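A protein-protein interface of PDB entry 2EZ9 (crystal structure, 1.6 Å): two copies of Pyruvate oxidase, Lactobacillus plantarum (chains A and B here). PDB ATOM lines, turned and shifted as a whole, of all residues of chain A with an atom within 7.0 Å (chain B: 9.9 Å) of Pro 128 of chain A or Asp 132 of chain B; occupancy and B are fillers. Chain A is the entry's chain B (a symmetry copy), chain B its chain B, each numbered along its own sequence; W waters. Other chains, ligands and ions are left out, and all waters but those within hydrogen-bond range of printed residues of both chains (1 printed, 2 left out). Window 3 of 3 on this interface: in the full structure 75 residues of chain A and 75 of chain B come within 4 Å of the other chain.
The side-chain carboxylate (OD2) of Asp 132 of chain B is in salt-bridge range of the guanidinium group (NH1) of Arg 98 of chain B. The side-chain hydroxyl (OH) of Tyr 95 of chain B is in hydrogen-bond range of the side-chain carboxylate (OD2) of Asp 132 of chain B. NE of Arg 98 of chain B lies within salt-bridge range of OE2 of Glu 99 of chain B (2.9 Å).
Among the printed residues, pairs that only touch across the chains: Pro 128 of chain A with Asp 132 of chain B (3.3 Å), Asp 132 of chain A with Pro 128 of chain B (3.3 Å), Ile 129 of chain A with Tyr 95 of chain B (3.5 Å), Ile 129 of chain A with Asp 132 of chain B (3.6 Å), Asp 132 of chain A with Ile 129 of chain B (3.6 Å), Met 124 of chain A with Phe 419 of chain B (3.8 Å) and Met 124 of chain A with Arg 98 of chain B (3.99 Å).
Of the printed residues of chain B, Pro 128 of chain A touches Asp 132. Asp 132 of chain B touches just these residues of chain A: Pro 128 and Ile 129. No residue of chain B comes within 4 Å of Asn 127 of chain A. Of chain B, only Tyr 95 (3.5 Å) and Asp 132 (3.6 Å) come within 4 Å of Ile 129 of chain A. Printed residues of chain A within 4 Å of Phe 419 of chain B: Met 124 (3.8 Å). Of the printed residues of chain A, Pro 128 of chain B touches Asp 132 (3.3 Å). Of the printed residues of chain B, Asp 132 of chain A touches Pro 128 (3.3 Å) and Ile 129 (3.6 Å). Of the printed residues of chain A, Tyr 95 of chain B touches Ile 129. Printed residues of chain B within 4 Å of Met 124 of chain A: Arg 98 and Phe 419. Thr 139 of chain A touches none of the printed residues of chain B. The nearest printed residue of chain A that does not touch Pro 128 of chain B is Pro 128 of chain A (5.5 Å).
Of the 13 printed residues of chain A, 4 touch a printed residue of chain B. Hydrophobic or aromatic side chains of chain A within 4 Å of the printed part of chain B: Met 124, Pro 128 and Ile 129. Printed residues of chain B that touch a printed residue of chain A: Tyr 95, Arg 98, Pro 128, Ile 129, Asp 132 and Phe 419. Along chain B the printed residues that touch a printed residue of chain A span positions 95 to 419. Among the printed residues, 7 pairs touch across the chains. Among the printed residues, no Asp or Glu carboxylate lies within 4 Å of a Lys or Arg side-chain nitrogen of the other chain.
Pro 128 of chain A touches Asp 132 of chain B, and with the chains exchanged Asp 132 of chain A touches Pro 128 of chain B. Ile 129 of chain A touches Asp 132 of chain B, and with the chains exchanged Asp 132 of chain A touches Ile 129 of chain B. 10 positions are printed for both chains. Of the 7 pairs that touch across the chains among the printed residues, 4 have their exchanged pair printed and touching as well.
Water W1 lies within hydrogen-bond range of OD2 of Asp 132 of chain B (2.7 Å), O of Asn 125 of chain A (2.8 Å) and NH2 of Arg 98 of chain B (2.9 Å).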
ATOM      1  N   MET A  91      20.291   5.213 -14.091  1.00  0.00           N
ATOM      2  CA  MET A  91      21.552   5.072 -14.820  1.00  0.00           C
ATOM      3  C   MET A  91      21.474   4.402 -16.186  1.00  0.00           C
ATOM      4  O   MET A  91      22.054   4.910 -17.158  1.00  0.00           O
ATOM      5  CB  MET A  91      22.628   4.413 -13.944  1.00  0.00           C
ATOM      6  CG  MET A  91      23.100   5.326 -12.863  1.00  0.00           C
ATOM      7  SD  MET A  91      23.879   6.789 -13.560  1.00  0.00           S
ATOM      8  CE  MET A  91      24.489   7.522 -12.045  1.00  0.00           C
ATOM      9  N   MET A 124      23.825  12.015   0.859  1.00  0.00           N
ATOM     10  CA  MET A 124      25.196  11.799   0.431  1.00  0.00           C
ATOM     11  C   MET A 124      25.530  12.907  -0.549  1.00  0.00           C
ATOM     12  O   MET A 124      24.630  13.621  -1.028  1.00  0.00           O
ATOM     13  CB  MET A 124      25.337  10.428  -0.245  1.00  0.00           C
ATOM     14  CG  MET A 124      24.575  10.305  -1.560  1.00  0.00           C
ATOM     15  SD  MET A 124      23.871   8.662  -1.848  1.00  0.00           S
ATOM     16  CE  MET A 124      22.506   8.653  -0.660  1.00  0.00           C
ATOM     17  N   ASN A 125      26.823  13.046  -0.855  1.00  0.00           N
ATOM     18  CA  ASN A 125      27.243  13.930  -1.919  1.00  0.00           C
ATOM     19  C   ASN A 125      26.853  13.272  -3.241  1.00  0.00           C
ATOM     20  O   ASN A 125      27.470  12.293  -3.673  1.00  0.00           O
ATOM     21  CB  ASN A 125      28.751  14.212  -1.846  1.00  0.00           C
ATOM     22  CG  ASN A 125      29.248  15.039  -3.020  1.00  0.00           C
ATOM     23  OD1 ASN A 125      28.462  15.660  -3.749  1.00  0.00           O
ATOM     24  ND2 ASN A 125      30.554  15.051  -3.214  1.00  0.00           N
ATOM     25  N   GLU A 126      25.809  13.795  -3.878  1.00  0.00           N
ATOM     26  CA  GLU A 126      25.303  13.147  -5.085  1.00  0.00           C
ATOM     27  C   GLU A 126      26.011  13.555  -6.365  1.00  0.00           C
ATOM     28  O   GLU A 126      25.868  12.884  -7.390  1.00  0.00           O
ATOM     29  CB  GLU A 126      23.803  13.388  -5.228  1.00  0.00           C
ATOM     30  CG  GLU A 126      23.002  12.638  -4.182  1.00  0.00           C
ATOM     31  CD  GLU A 126      21.518  12.798  -4.400  1.00  0.00           C
ATOM     32  OE1 GLU A 126      21.016  13.926  -4.216  1.00  0.00           O
ATOM     33  OE2 GLU A 126      20.867  11.795  -4.736  1.00  0.00           O
ATOM     34  N   ASN A 127      26.777  14.643  -6.315  1.00  0.00           N
ATOM     35  CA  ASN A 127      27.387  15.153  -7.544  1.00  0.00           C
ATOM     36  C   ASN A 127      28.355  14.175  -8.245  1.00  0.00           C
ATOM     37  O   ASN A 127      28.288  14.007  -9.460  1.00  0.00           O
ATOM     38  CB  ASN A 127      28.022  16.530  -7.302  1.00  0.00           C
ATOM     39  CG  ASN A 127      28.445  17.203  -8.597  1.00  0.00           C
ATOM     40  OD1 ASN A 127      29.626  17.188  -8.954  1.00  0.00           O
ATOM     41  ND2 ASN A 127      27.477  17.764  -9.325  1.00  0.00           N
ATOM     42  N   PRO A 128      29.242  13.497  -7.489  1.00  0.00           N
ATOM     43  CA  PRO A 128      30.140  12.514  -8.157  1.00  0.00           C
ATOM     44  C   PRO A 128      29.427  11.340  -8.823  1.00  0.00           C
ATOM     45  O   PRO A 128      30.010  10.691  -9.684  1.00  0.00           O
ATOM     46  CB  PRO A 128      30.991  11.968  -7.014  1.00  0.00           C
ATOM     47  CG  PRO A 128      30.864  12.954  -5.908  1.00  0.00           C
ATOM     48  CD  PRO A 128      29.518  13.604  -6.040  1.00  0.00           C
ATOM     49  N   ILE A 129      28.191  11.052  -8.420  1.00  0.00           N
ATOM     50  CA  ILE A 129      27.454   9.913  -8.980  1.00  0.00           C
ATOM     51  C   ILE A 129      27.233  10.072 -10.493  1.00  0.00           C
ATOM     52  O   ILE A 129      27.305   9.085 -11.250  1.00  0.00           O
ATOM     53  CB  ILE A 129      26.094   9.742  -8.275  1.00  0.00           C
ATOM     54  CG1 ILE A 129      26.310   9.536  -6.765  1.00  0.00           C
ATOM     55  CG2 ILE A 129      25.317   8.565  -8.873  1.00  0.00           C
ATOM     56  CD1 ILE A 129      25.016   9.457  -5.957  1.00  0.00           C
ATOM     57  N   TYR A 130      26.983  11.320 -10.912  1.00  0.00           N
ATOM     58  CA  TYR A 130      26.566  11.642 -12.290  1.00  0.00           C
ATOM     59  C   TYR A 130      27.656  12.265 -13.155  1.00  0.00           C
ATOM     60  O   TYR A 130      27.410  12.589 -14.319  1.00  0.00           O
ATOM     61  CB  TYR A 130      25.302  12.542 -12.257  1.00  0.00           C
ATOM     62  CG  TYR A 130      24.219  11.852 -11.470  1.00  0.00           C
ATOM     63  CD1 TYR A 130      23.410  10.895 -12.076  1.00  0.00           C
ATOM     64  CD2 TYR A 130      24.059  12.094 -10.091  1.00  0.00           C
ATOM     65  CE1 TYR A 130      22.453  10.204 -11.352  1.00  0.00           C
ATOM     66  CE2 TYR A 130      23.104  11.414  -9.362  1.00  0.00           C
ATOM     67  CZ  TYR A 130      22.310  10.467 -10.005  1.00  0.00           C
ATOM     68  OH  TYR A 130      21.369   9.765  -9.307  1.00  0.00           O
ATOM     69  N   ALA A 131      28.858  12.412 -12.595  1.00  0.00           N
ATOM     70  CA  ALA A 131      29.947  13.086 -13.309  1.00  0.00           C
ATOM     71  C   ALA A 131      30.325  12.411 -14.625  1.00  0.00           C
ATOM     72  O   ALA A 131      30.624  13.085 -15.614  1.00  0.00           O
ATOM     73  CB  ALA A 131      31.181  13.214 -12.396  1.00  0.00           C
ATOM     74  N   ASP A 132      30.312  11.083 -14.650  1.00  0.00           N
ATOM     75  CA  ASP A 132      30.734  10.389 -15.862  1.00  0.00           C
ATOM     76  C   ASP A 132      29.682  10.415 -16.975  1.00  0.00           C
ATOM     77  O   ASP A 132      30.026  10.605 -18.152  1.00  0.00           O
ATOM     78  CB  ASP A 132      31.121   8.947 -15.558  1.00  0.00           C
ATOM     79  CG  ASP A 132      31.549   8.210 -16.799  1.00  0.00           C
ATOM     80  OD1 ASP A 132      32.630   8.551 -17.341  1.00  0.00           O
ATOM     81  OD2 ASP A 132      30.780   7.329 -17.245  1.00  0.00           O
ATOM     82  N   ASN A 137      26.486  18.781 -14.994  1.00  0.00           N
ATOM     83  CA  ASN A 137      26.250  18.048 -13.749  1.00  0.00           C
ATOM     84  C   ASN A 137      26.452  18.937 -12.545  1.00  0.00           C
ATOM     85  O   ASN A 137      27.577  19.139 -12.117  1.00  0.00           O
ATOM     86  CB  ASN A 137      27.199  16.839 -13.670  1.00  0.00           C
ATOM     87  CG  ASN A 137      27.069  16.087 -12.358  1.00  0.00           C
ATOM     88  OD1 ASN A 137      25.958  15.883 -11.860  1.00  0.00           O
ATOM     89  ND2 ASN A 137      28.200  15.658 -11.804  1.00  0.00           N
ATOM     90  N   THR A 139      24.877  20.663  -8.624  1.00  0.00           N
ATOM     91  CA  THR A 139      23.961  20.694  -7.488  1.00  0.00           C
ATOM     92  C   THR A 139      23.525  22.143  -7.311  1.00  0.00           C
ATOM     93  O   THR A 139      24.364  23.028  -7.108  1.00  0.00           O
ATOM     94  CB  THR A 139      24.634  20.181  -6.176  1.00  0.00           C
ATOM     95  OG1 THR A 139      24.979  18.787  -6.304  1.00  0.00           O
ATOM     96  CG2 THR A 139      23.675  20.353  -4.985  1.00  0.00           C
ATOM     97  N   GLN A 167      21.043  18.203  -9.453  1.00  0.00           N
ATOM     98  CA  GLN A 167      20.636  17.759  -8.110  1.00  0.00           C
ATOM     99  C   GLN A 167      19.991  18.937  -7.398  1.00  0.00           C
ATOM    100  O   GLN A 167      20.590  20.021  -7.307  1.00  0.00           O
ATOM    101  CB  GLN A 167      21.828  17.213  -7.302  1.00  0.00           C
ATOM    102  CG  GLN A 167      22.549  16.021  -7.978  1.00  0.00           C
ATOM    103  CD  GLN A 167      23.773  16.421  -8.821  1.00  0.00           C
ATOM    104  OE1 GLN A 167      24.555  17.293  -8.441  1.00  0.00           O
ATOM    105  NE2 GLN A 167      23.932  15.775  -9.965  1.00  0.00           N
ATOM    106  N   MET B  91      24.209  -0.779  -9.578  1.00  0.00           N
ATOM    107  CA  MET B  91      24.395   0.399  -8.729  1.00  0.00           C
ATOM    108  C   MET B  91      23.590   0.437  -7.436  1.00  0.00           C
ATOM    109  O   MET B  91      24.146   0.742  -6.370  1.00  0.00           O
ATOM    110  CB  MET B  91      24.209   1.695  -9.531  1.00  0.00           C
ATOM    111  CG  MET B  91      25.336   1.929 -10.479  1.00  0.00           C
ATOM    112  SD  MET B  91      26.885   2.133  -9.590  1.00  0.00           S
ATOM    113  CE  MET B  91      27.934   2.589 -10.966  1.00  0.00           C
ATOM    114  N   LEU B  94      25.230  -1.803  -4.977  1.00  0.00           N
ATOM    115  CA  LEU B  94      26.573  -1.363  -4.601  1.00  0.00           C
ATOM    116  C   LEU B  94      26.515  -0.189  -3.634  1.00  0.00           C
ATOM    117  O   LEU B  94      27.235  -0.161  -2.625  1.00  0.00           O
ATOM    118  CB  LEU B  94      27.427  -1.023  -5.831  1.00  0.00           C
ATOM    119  CG  LEU B  94      27.683  -2.194  -6.792  1.00  0.00           C
ATOM    120  CD1 LEU B  94      28.682  -1.780  -7.849  1.00  0.00           C
ATOM    121  CD2 LEU B  94      28.177  -3.454  -6.044  1.00  0.00           C
ATOM    122  N   TYR B  95      25.646   0.778  -3.929  1.00  0.00           N
ATOM    123  CA  TYR B  95      25.429   1.886  -2.982  1.00  0.00           C
ATOM    124  C   TYR B  95      24.882   1.407  -1.639  1.00  0.00           C
ATOM    125  O   TYR B  95      25.253   1.947  -0.590  1.00  0.00           O
ATOM    126  CB  TYR B  95      24.553   3.002  -3.597  1.00  0.00           C
ATOM    127  CG  TYR B  95      25.396   3.927  -4.439  1.00  0.00           C
ATOM    128  CD1 TYR B  95      26.006   5.048  -3.872  1.00  0.00           C
ATOM    129  CD2 TYR B  95      25.630   3.652  -5.790  1.00  0.00           C
ATOM    130  CE1 TYR B  95      26.823   5.889  -4.631  1.00  0.00           C
ATOM    131  CE2 TYR B  95      26.451   4.484  -6.561  1.00  0.00           C
ATOM    132  CZ  TYR B  95      27.049   5.594  -5.965  1.00  0.00           C
ATOM    133  OH  TYR B  95      27.878   6.394  -6.720  1.00  0.00           O
ATOM    134  N   ALA B  97      25.556  -1.452  -0.285  1.00  0.00           N
ATOM    135  CA  ALA B  97      26.701  -2.027   0.428  1.00  0.00           C
ATOM    136  C   ALA B  97      27.629  -0.928   0.979  1.00  0.00           C
ATOM    137  O   ALA B  97      28.145  -1.035   2.088  1.00  0.00           O
ATOM    138  CB  ALA B  97      27.459  -2.993  -0.487  1.00  0.00           C
ATOM    139  N   ARG B  98      27.847   0.123   0.202  1.00  0.00           N
ATOM    140  CA  ARG B  98      28.669   1.226   0.682  1.00  0.00           C
ATOM    141  C   ARG B  98      28.082   1.871   1.927  1.00  0.00           C
ATOM    142  O   ARG B  98      28.781   2.079   2.930  1.00  0.00           O
ATOM    143  CB  ARG B  98      28.852   2.301  -0.384  1.00  0.00           C
ATOM    144  CG  ARG B  98      29.811   3.383   0.091  1.00  0.00           C
ATOM    145  CD  ARG B  98      29.930   4.538  -0.893  1.00  0.00           C
ATOM    146  NE  ARG B  98      28.807   5.479  -0.802  1.00  0.00           N
ATOM    147  CZ  ARG B  98      28.658   6.544  -1.585  1.00  0.00           C
ATOM    148  NH1 ARG B  98      29.555   6.825  -2.527  1.00  0.00           N
ATOM    149  NH2 ARG B  98      27.609   7.345  -1.423  1.00  0.00           N
ATOM    150  N   GLU B  99      26.800   2.193   1.853  1.00  0.00           N
ATOM    151  CA  GLU B  99      26.145   2.933   2.935  1.00  0.00           C
ATOM    152  C   GLU B  99      25.928   2.098   4.196  1.00  0.00           C
ATOM    153  O   GLU B  99      25.981   2.632   5.310  1.00  0.00           O
ATOM    154  CB  GLU B  99      24.832   3.554   2.445  1.00  0.00           C
ATOM    155  CG  GLU B  99      25.049   4.612   1.356  1.00  0.00           C
ATOM    156  CD  GLU B  99      25.841   5.818   1.849  1.00  0.00           C
ATOM    157  OE1 GLU B  99      25.490   6.390   2.908  1.00  0.00           O
ATOM    158  OE2 GLU B  99      26.815   6.211   1.174  1.00  0.00           O
ATOM    159  N   GLU B 126      35.155   2.435 -18.425  1.00  0.00           N
ATOM    160  CA  GLU B 126      34.252   2.074 -17.335  1.00  0.00           C
ATOM    161  C   GLU B 126      34.721   2.509 -15.957  1.00  0.00           C
ATOM    162  O   GLU B 126      33.931   2.512 -15.009  1.00  0.00           O
ATOM    163  CB  GLU B 126      33.990   0.571 -17.338  1.00  0.00           C
ATOM    164  CG  GLU B 126      33.145   0.141 -18.521  1.00  0.00           C
ATOM    165  CD  GLU B 126      32.804  -1.327 -18.454  1.00  0.00           C
ATOM    166  OE1 GLU B 126      33.729  -2.152 -18.603  1.00  0.00           O
ATOM    167  OE2 GLU B 126      31.616  -1.641 -18.270  1.00  0.00           O
ATOM    168  N   ASN B 127      35.994   2.882 -15.839  1.00  0.00           N
ATOM    169  CA  ASN B 127      36.533   3.194 -14.514  1.00  0.00           C
ATOM    170  C   ASN B 127      35.840   4.371 -13.790  1.00  0.00           C
ATOM    171  O   ASN B 127      35.528   4.267 -12.606  1.00  0.00           O
ATOM    172  CB  ASN B 127      38.058   3.366 -14.577  1.00  0.00           C
ATOM    173  CG  ASN B 127      38.684   3.445 -13.195  1.00  0.00           C
ATOM    174  OD1 ASN B 127      39.004   4.534 -12.713  1.00  0.00           O
ATOM    175  ND2 ASN B 127      38.828   2.293 -12.535  1.00  0.00           N
ATOM    176  N   PRO B 128      35.563   5.485 -14.496  1.00  0.00           N
ATOM    177  CA  PRO B 128      34.847   6.599 -13.812  1.00  0.00           C
ATOM    178  C   PRO B 128      33.443   6.256 -13.322  1.00  0.00           C
ATOM    179  O   PRO B 128      32.921   6.949 -12.456  1.00  0.00           O
ATOM    180  CB  PRO B 128      34.726   7.667 -14.895  1.00  0.00           C
ATOM    181  CG  PRO B 128      35.736   7.314 -15.928  1.00  0.00           C
ATOM    182  CD  PRO B 128      35.910   5.824 -15.893  1.00  0.00           C
ATOM    183  N   ILE B 129      32.825   5.216 -13.878  1.00  0.00           N
ATOM    184  CA  ILE B 129      31.458   4.847 -13.493  1.00  0.00           C
ATOM    185  C   ILE B 129      31.373   4.469 -12.005  1.00  0.00           C
ATOM    186  O   ILE B 129      30.382   4.798 -11.325  1.00  0.00           O
ATOM    187  CB  ILE B 129      30.944   3.676 -14.354  1.00  0.00           C
ATOM    188  CG1 ILE B 129      30.983   4.064 -15.843  1.00  0.00           C
ATOM    189  CG2 ILE B 129      29.525   3.279 -13.938  1.00  0.00           C
ATOM    190  CD1 ILE B 129      30.589   2.933 -16.790  1.00  0.00           C
ATOM    191  N   TYR B 130      32.425   3.795 -11.520  1.00  0.00           N
ATOM    192  CA  TYR B 130      32.446   3.190 -10.175  1.00  0.00           C
ATOM    193  C   TYR B 130      33.283   3.948  -9.150  1.00  0.00           C
ATOM    194  O   TYR B 130      33.384   3.519  -7.998  1.00  0.00           O
ATOM    195  CB  TYR B 130      32.900   1.709 -10.276  1.00  0.00           C
ATOM    196  CG  TYR B 130      31.993   0.973 -11.228  1.00  0.00           C
ATOM    197  CD1 TYR B 130      30.769   0.474 -10.790  1.00  0.00           C
ATOM    198  CD2 TYR B 130      32.321   0.852 -12.592  1.00  0.00           C
ATOM    199  CE1 TYR B 130      29.896  -0.146 -11.666  1.00  0.00           C
ATOM    200  CE2 TYR B 130      31.458   0.229 -13.472  1.00  0.00           C
ATOM    201  CZ  TYR B 130      30.244  -0.261 -12.996  1.00  0.00           C
ATOM    202  OH  TYR B 130      29.362  -0.866 -13.845  1.00  0.00           O
ATOM    203  N   ALA B 131      33.863   5.076  -9.562  1.00  0.00           N
ATOM    204  CA  ALA B 131      34.763   5.828  -8.684  1.00  0.00           C
ATOM    205  C   ALA B 131      34.103   6.301  -7.391  1.00  0.00           C
ATOM    206  O   ALA B 131      34.725   6.286  -6.326  1.00  0.00           O
ATOM    207  CB  ALA B 131      35.373   7.021  -9.443  1.00  0.00           C
ATOM    208  N   ASP B 132      32.845   6.718  -7.472  1.00  0.00           N
ATOM    209  CA  ASP B 132      32.191   7.247  -6.278  1.00  0.00           C
ATOM    210  C   ASP B 132      31.762   6.159  -5.289  1.00  0.00           C
ATOM    211  O   ASP B 132      31.921   6.330  -4.070  1.00  0.00           O
ATOM    212  CB  ASP B 132      30.987   8.103  -6.650  1.00  0.00           C
ATOM    213  CG  ASP B 132      30.292   8.649  -5.432  1.00  0.00           C
ATOM    214  OD1 ASP B 132      30.896   9.514  -4.750  1.00  0.00           O
ATOM    215  OD2 ASP B 132      29.170   8.175  -5.143  1.00  0.00           O
ATOM    216  N   VAL B 133      31.247   5.043  -5.806  1.00  0.00           N
ATOM    217  CA  VAL B 133      30.684   4.006  -4.927  1.00  0.00           C
ATOM    218  C   VAL B 133      31.758   3.144  -4.262  1.00  0.00           C
ATOM    219  O   VAL B 133      31.541   2.606  -3.178  1.00  0.00           O
ATOM    220  CB  VAL B 133      29.659   3.106  -5.676  1.00  0.00           C
ATOM    221  CG1 VAL B 133      30.362   2.160  -6.633  1.00  0.00           C
ATOM    222  CG2 VAL B 133      28.799   2.320  -4.677  1.00  0.00           C
ATOM    223  N   ALA B 134      32.915   3.037  -4.915  1.00  0.00           N
ATOM    224  CA  ALA B 134      33.912   2.020  -4.577  1.00  0.00           C
ATOM    225  C   ALA B 134      35.033   2.523  -3.670  1.00  0.00           C
ATOM    226  O   ALA B 134      35.564   3.625  -3.859  1.00  0.00           O
ATOM    227  CB  ALA B 134      34.498   1.445  -5.868  1.00  0.00           C
ATOM    228  N   ASP B 135      35.411   1.693  -2.702  1.00  0.00           N
ATOM    229  CA  ASP B 135      36.622   1.903  -1.924  1.00  0.00           C
ATOM    230  C   ASP B 135      37.863   1.604  -2.779  1.00  0.00           C
ATOM    231  O   ASP B 135      38.926   2.218  -2.599  1.00  0.00           O
ATOM    232  CB  ASP B 135      36.604   0.982  -0.698  1.00  0.00           C
ATOM    233  CG  ASP B 135      37.870   1.081   0.117  1.00  0.00           C
ATOM    234  OD1 ASP B 135      37.988   2.030   0.932  1.00  0.00           O
ATOM    235  OD2 ASP B 135      38.753   0.217  -0.081  1.00  0.00           O
ATOM    236  N   TYR B 136      37.731   0.628  -3.679  1.00  0.00           N
ATOM    237  CA  TYR B 136      38.826   0.200  -4.553  1.00  0.00           C
ATOM    238  C   TYR B 136      38.222   0.002  -5.933  1.00  0.00           C
ATOM    239  O   TYR B 136      37.174  -0.626  -6.069  1.00  0.00           O
ATOM    240  CB  TYR B 136      39.429  -1.096  -4.022  1.00  0.00           C
ATOM    241  CG  TYR B 136      40.609  -1.655  -4.796  1.00  0.00           C
ATOM    242  CD1 TYR B 136      41.843  -0.992  -4.815  1.00  0.00           C
ATOM    243  CD2 TYR B 136      40.511  -2.877  -5.457  1.00  0.00           C
ATOM    244  CE1 TYR B 136      42.935  -1.521  -5.500  1.00  0.00           C
ATOM    245  CE2 TYR B 136      41.606  -3.417  -6.151  1.00  0.00           C
ATOM    246  CZ  TYR B 136      42.808  -2.731  -6.156  1.00  0.00           C
ATOM    247  OH  TYR B 136      43.883  -3.256  -6.840  1.00  0.00           O
ATOM    248  N   ASN B 137      38.855   0.585  -6.946  1.00  0.00           N
ATOM    249  CA  ASN B 137      38.226   0.698  -8.263  1.00  0.00           C
ATOM    250  C   ASN B 137      39.258   0.694  -9.365  1.00  0.00           C
ATOM    251  O   ASN B 137      39.851   1.722  -9.651  1.00  0.00           O
ATOM    252  CB  ASN B 137      37.394   1.991  -8.332  1.00  0.00           C
ATOM    253  CG  ASN B 137      36.787   2.216  -9.705  1.00  0.00           C
ATOM    254  OD1 ASN B 137      36.299   1.274 -10.336  1.00  0.00           O
ATOM    255  ND2 ASN B 137      36.801   3.465 -10.164  1.00  0.00           N
ATOM    256  N   GLY B 162      33.521  -2.128   2.676  1.00  0.00           N
ATOM    257  CA  GLY B 162      32.835  -1.495   1.555  1.00  0.00           C
ATOM    258  C   GLY B 162      33.040  -2.241   0.256  1.00  0.00           C
ATOM    259  O   GLY B 162      33.364  -3.438   0.245  1.00  0.00           O
ATOM    260  N   VAL B 163      32.846  -1.512  -0.841  1.00  0.00           N
ATOM    261  CA  VAL B 163      32.778  -2.095  -2.182  1.00  0.00           C
ATOM    262  C   VAL B 163      34.117  -2.018  -2.920  1.00  0.00           C
ATOM    263  O   VAL B 163      34.761  -0.957  -2.957  1.00  0.00           O
ATOM    264  CB  VAL B 163      31.648  -1.427  -3.015  1.00  0.00           C
ATOM    265  CG1 VAL B 163      31.585  -2.015  -4.413  1.00  0.00           C
ATOM    266  CG2 VAL B 163      30.302  -1.587  -2.303  1.00  0.00           C
ATOM    267  N   ALA B 164      34.541  -3.155  -3.476  1.00  0.00           N
ATOM    268  CA  ALA B 164      35.701  -3.183  -4.359  1.00  0.00           C
ATOM    269  C   ALA B 164      35.211  -3.588  -5.731  1.00  0.00           C
ATOM    270  O   ALA B 164      34.485  -4.578  -5.856  1.00  0.00           O
ATOM    271  CB  ALA B 164      36.749  -4.184  -3.854  1.00  0.00           C
ATOM    272  N   VAL B 165      35.601  -2.817  -6.743  1.00  0.00           N
ATOM    273  CA  VAL B 165      35.172  -3.038  -8.115  1.00  0.00           C
ATOM    274  C   VAL B 165      36.390  -3.274  -8.989  1.00  0.00           C
ATOM    275  O   VAL B 165      37.361  -2.528  -8.919  1.00  0.00           O
ATOM    276  CB  VAL B 165      34.373  -1.826  -8.670  1.00  0.00           C
ATOM    277  CG1 VAL B 165      33.883  -2.106 -10.100  1.00  0.00           C
ATOM    278  CG2 VAL B 165      33.200  -1.471  -7.742  1.00  0.00           C
ATOM    279  N   GLN B 167      37.197  -3.924 -13.076  1.00  0.00           N
ATOM    280  CA  GLN B 167      36.797  -4.059 -14.486  1.00  0.00           C
ATOM    281  C   GLN B 167      37.781  -4.994 -15.170  1.00  0.00           C
ATOM    282  O   GLN B 167      39.002  -4.774 -15.110  1.00  0.00           O
ATOM    283  CB  GLN B 167      36.746  -2.695 -15.200  1.00  0.00           C
ATOM    284  CG  GLN B 167      35.777  -1.681 -14.544  1.00  0.00           C
ATOM    285  CD  GLN B 167      36.448  -0.723 -13.544  1.00  0.00           C
ATOM    286  OE1 GLN B 167      37.559  -0.239 -13.767  1.00  0.00           O
ATOM    287  NE2 GLN B 167      35.765  -0.453 -12.444  1.00  0.00           N
ATOM    288  N   PHE B 419      20.932   3.837   2.686  1.00  0.00           N
ATOM    289  CA  PHE B 419      20.630   4.182   1.297  1.00  0.00           C
ATOM    290  C   PHE B 419      19.134   4.016   1.079  1.00  0.00           C
ATOM    291  O   PHE B 419      18.524   4.744   0.299  1.00  0.00           O
ATOM    292  CB  PHE B 419      21.444   3.270   0.364  1.00  0.00           C
ATOM    293  CG  PHE B 419      21.472   3.708  -1.078  1.00  0.00           C
ATOM    294  CD1 PHE B 419      21.986   4.958  -1.435  1.00  0.00           C
ATOM    295  CD2 PHE B 419      21.021   2.849  -2.078  1.00  0.00           C
ATOM    296  CE1 PHE B 419      22.024   5.358  -2.789  1.00  0.00           C
ATOM    297  CE2 PHE B 419      21.061   3.224  -3.429  1.00  0.00           C
ATOM    298  CZ  PHE B 419      21.559   4.479  -3.781  1.00  0.00           C
HETATM  299  O   HOH W   1      27.703   9.544  -3.272  1.00  0.00           O
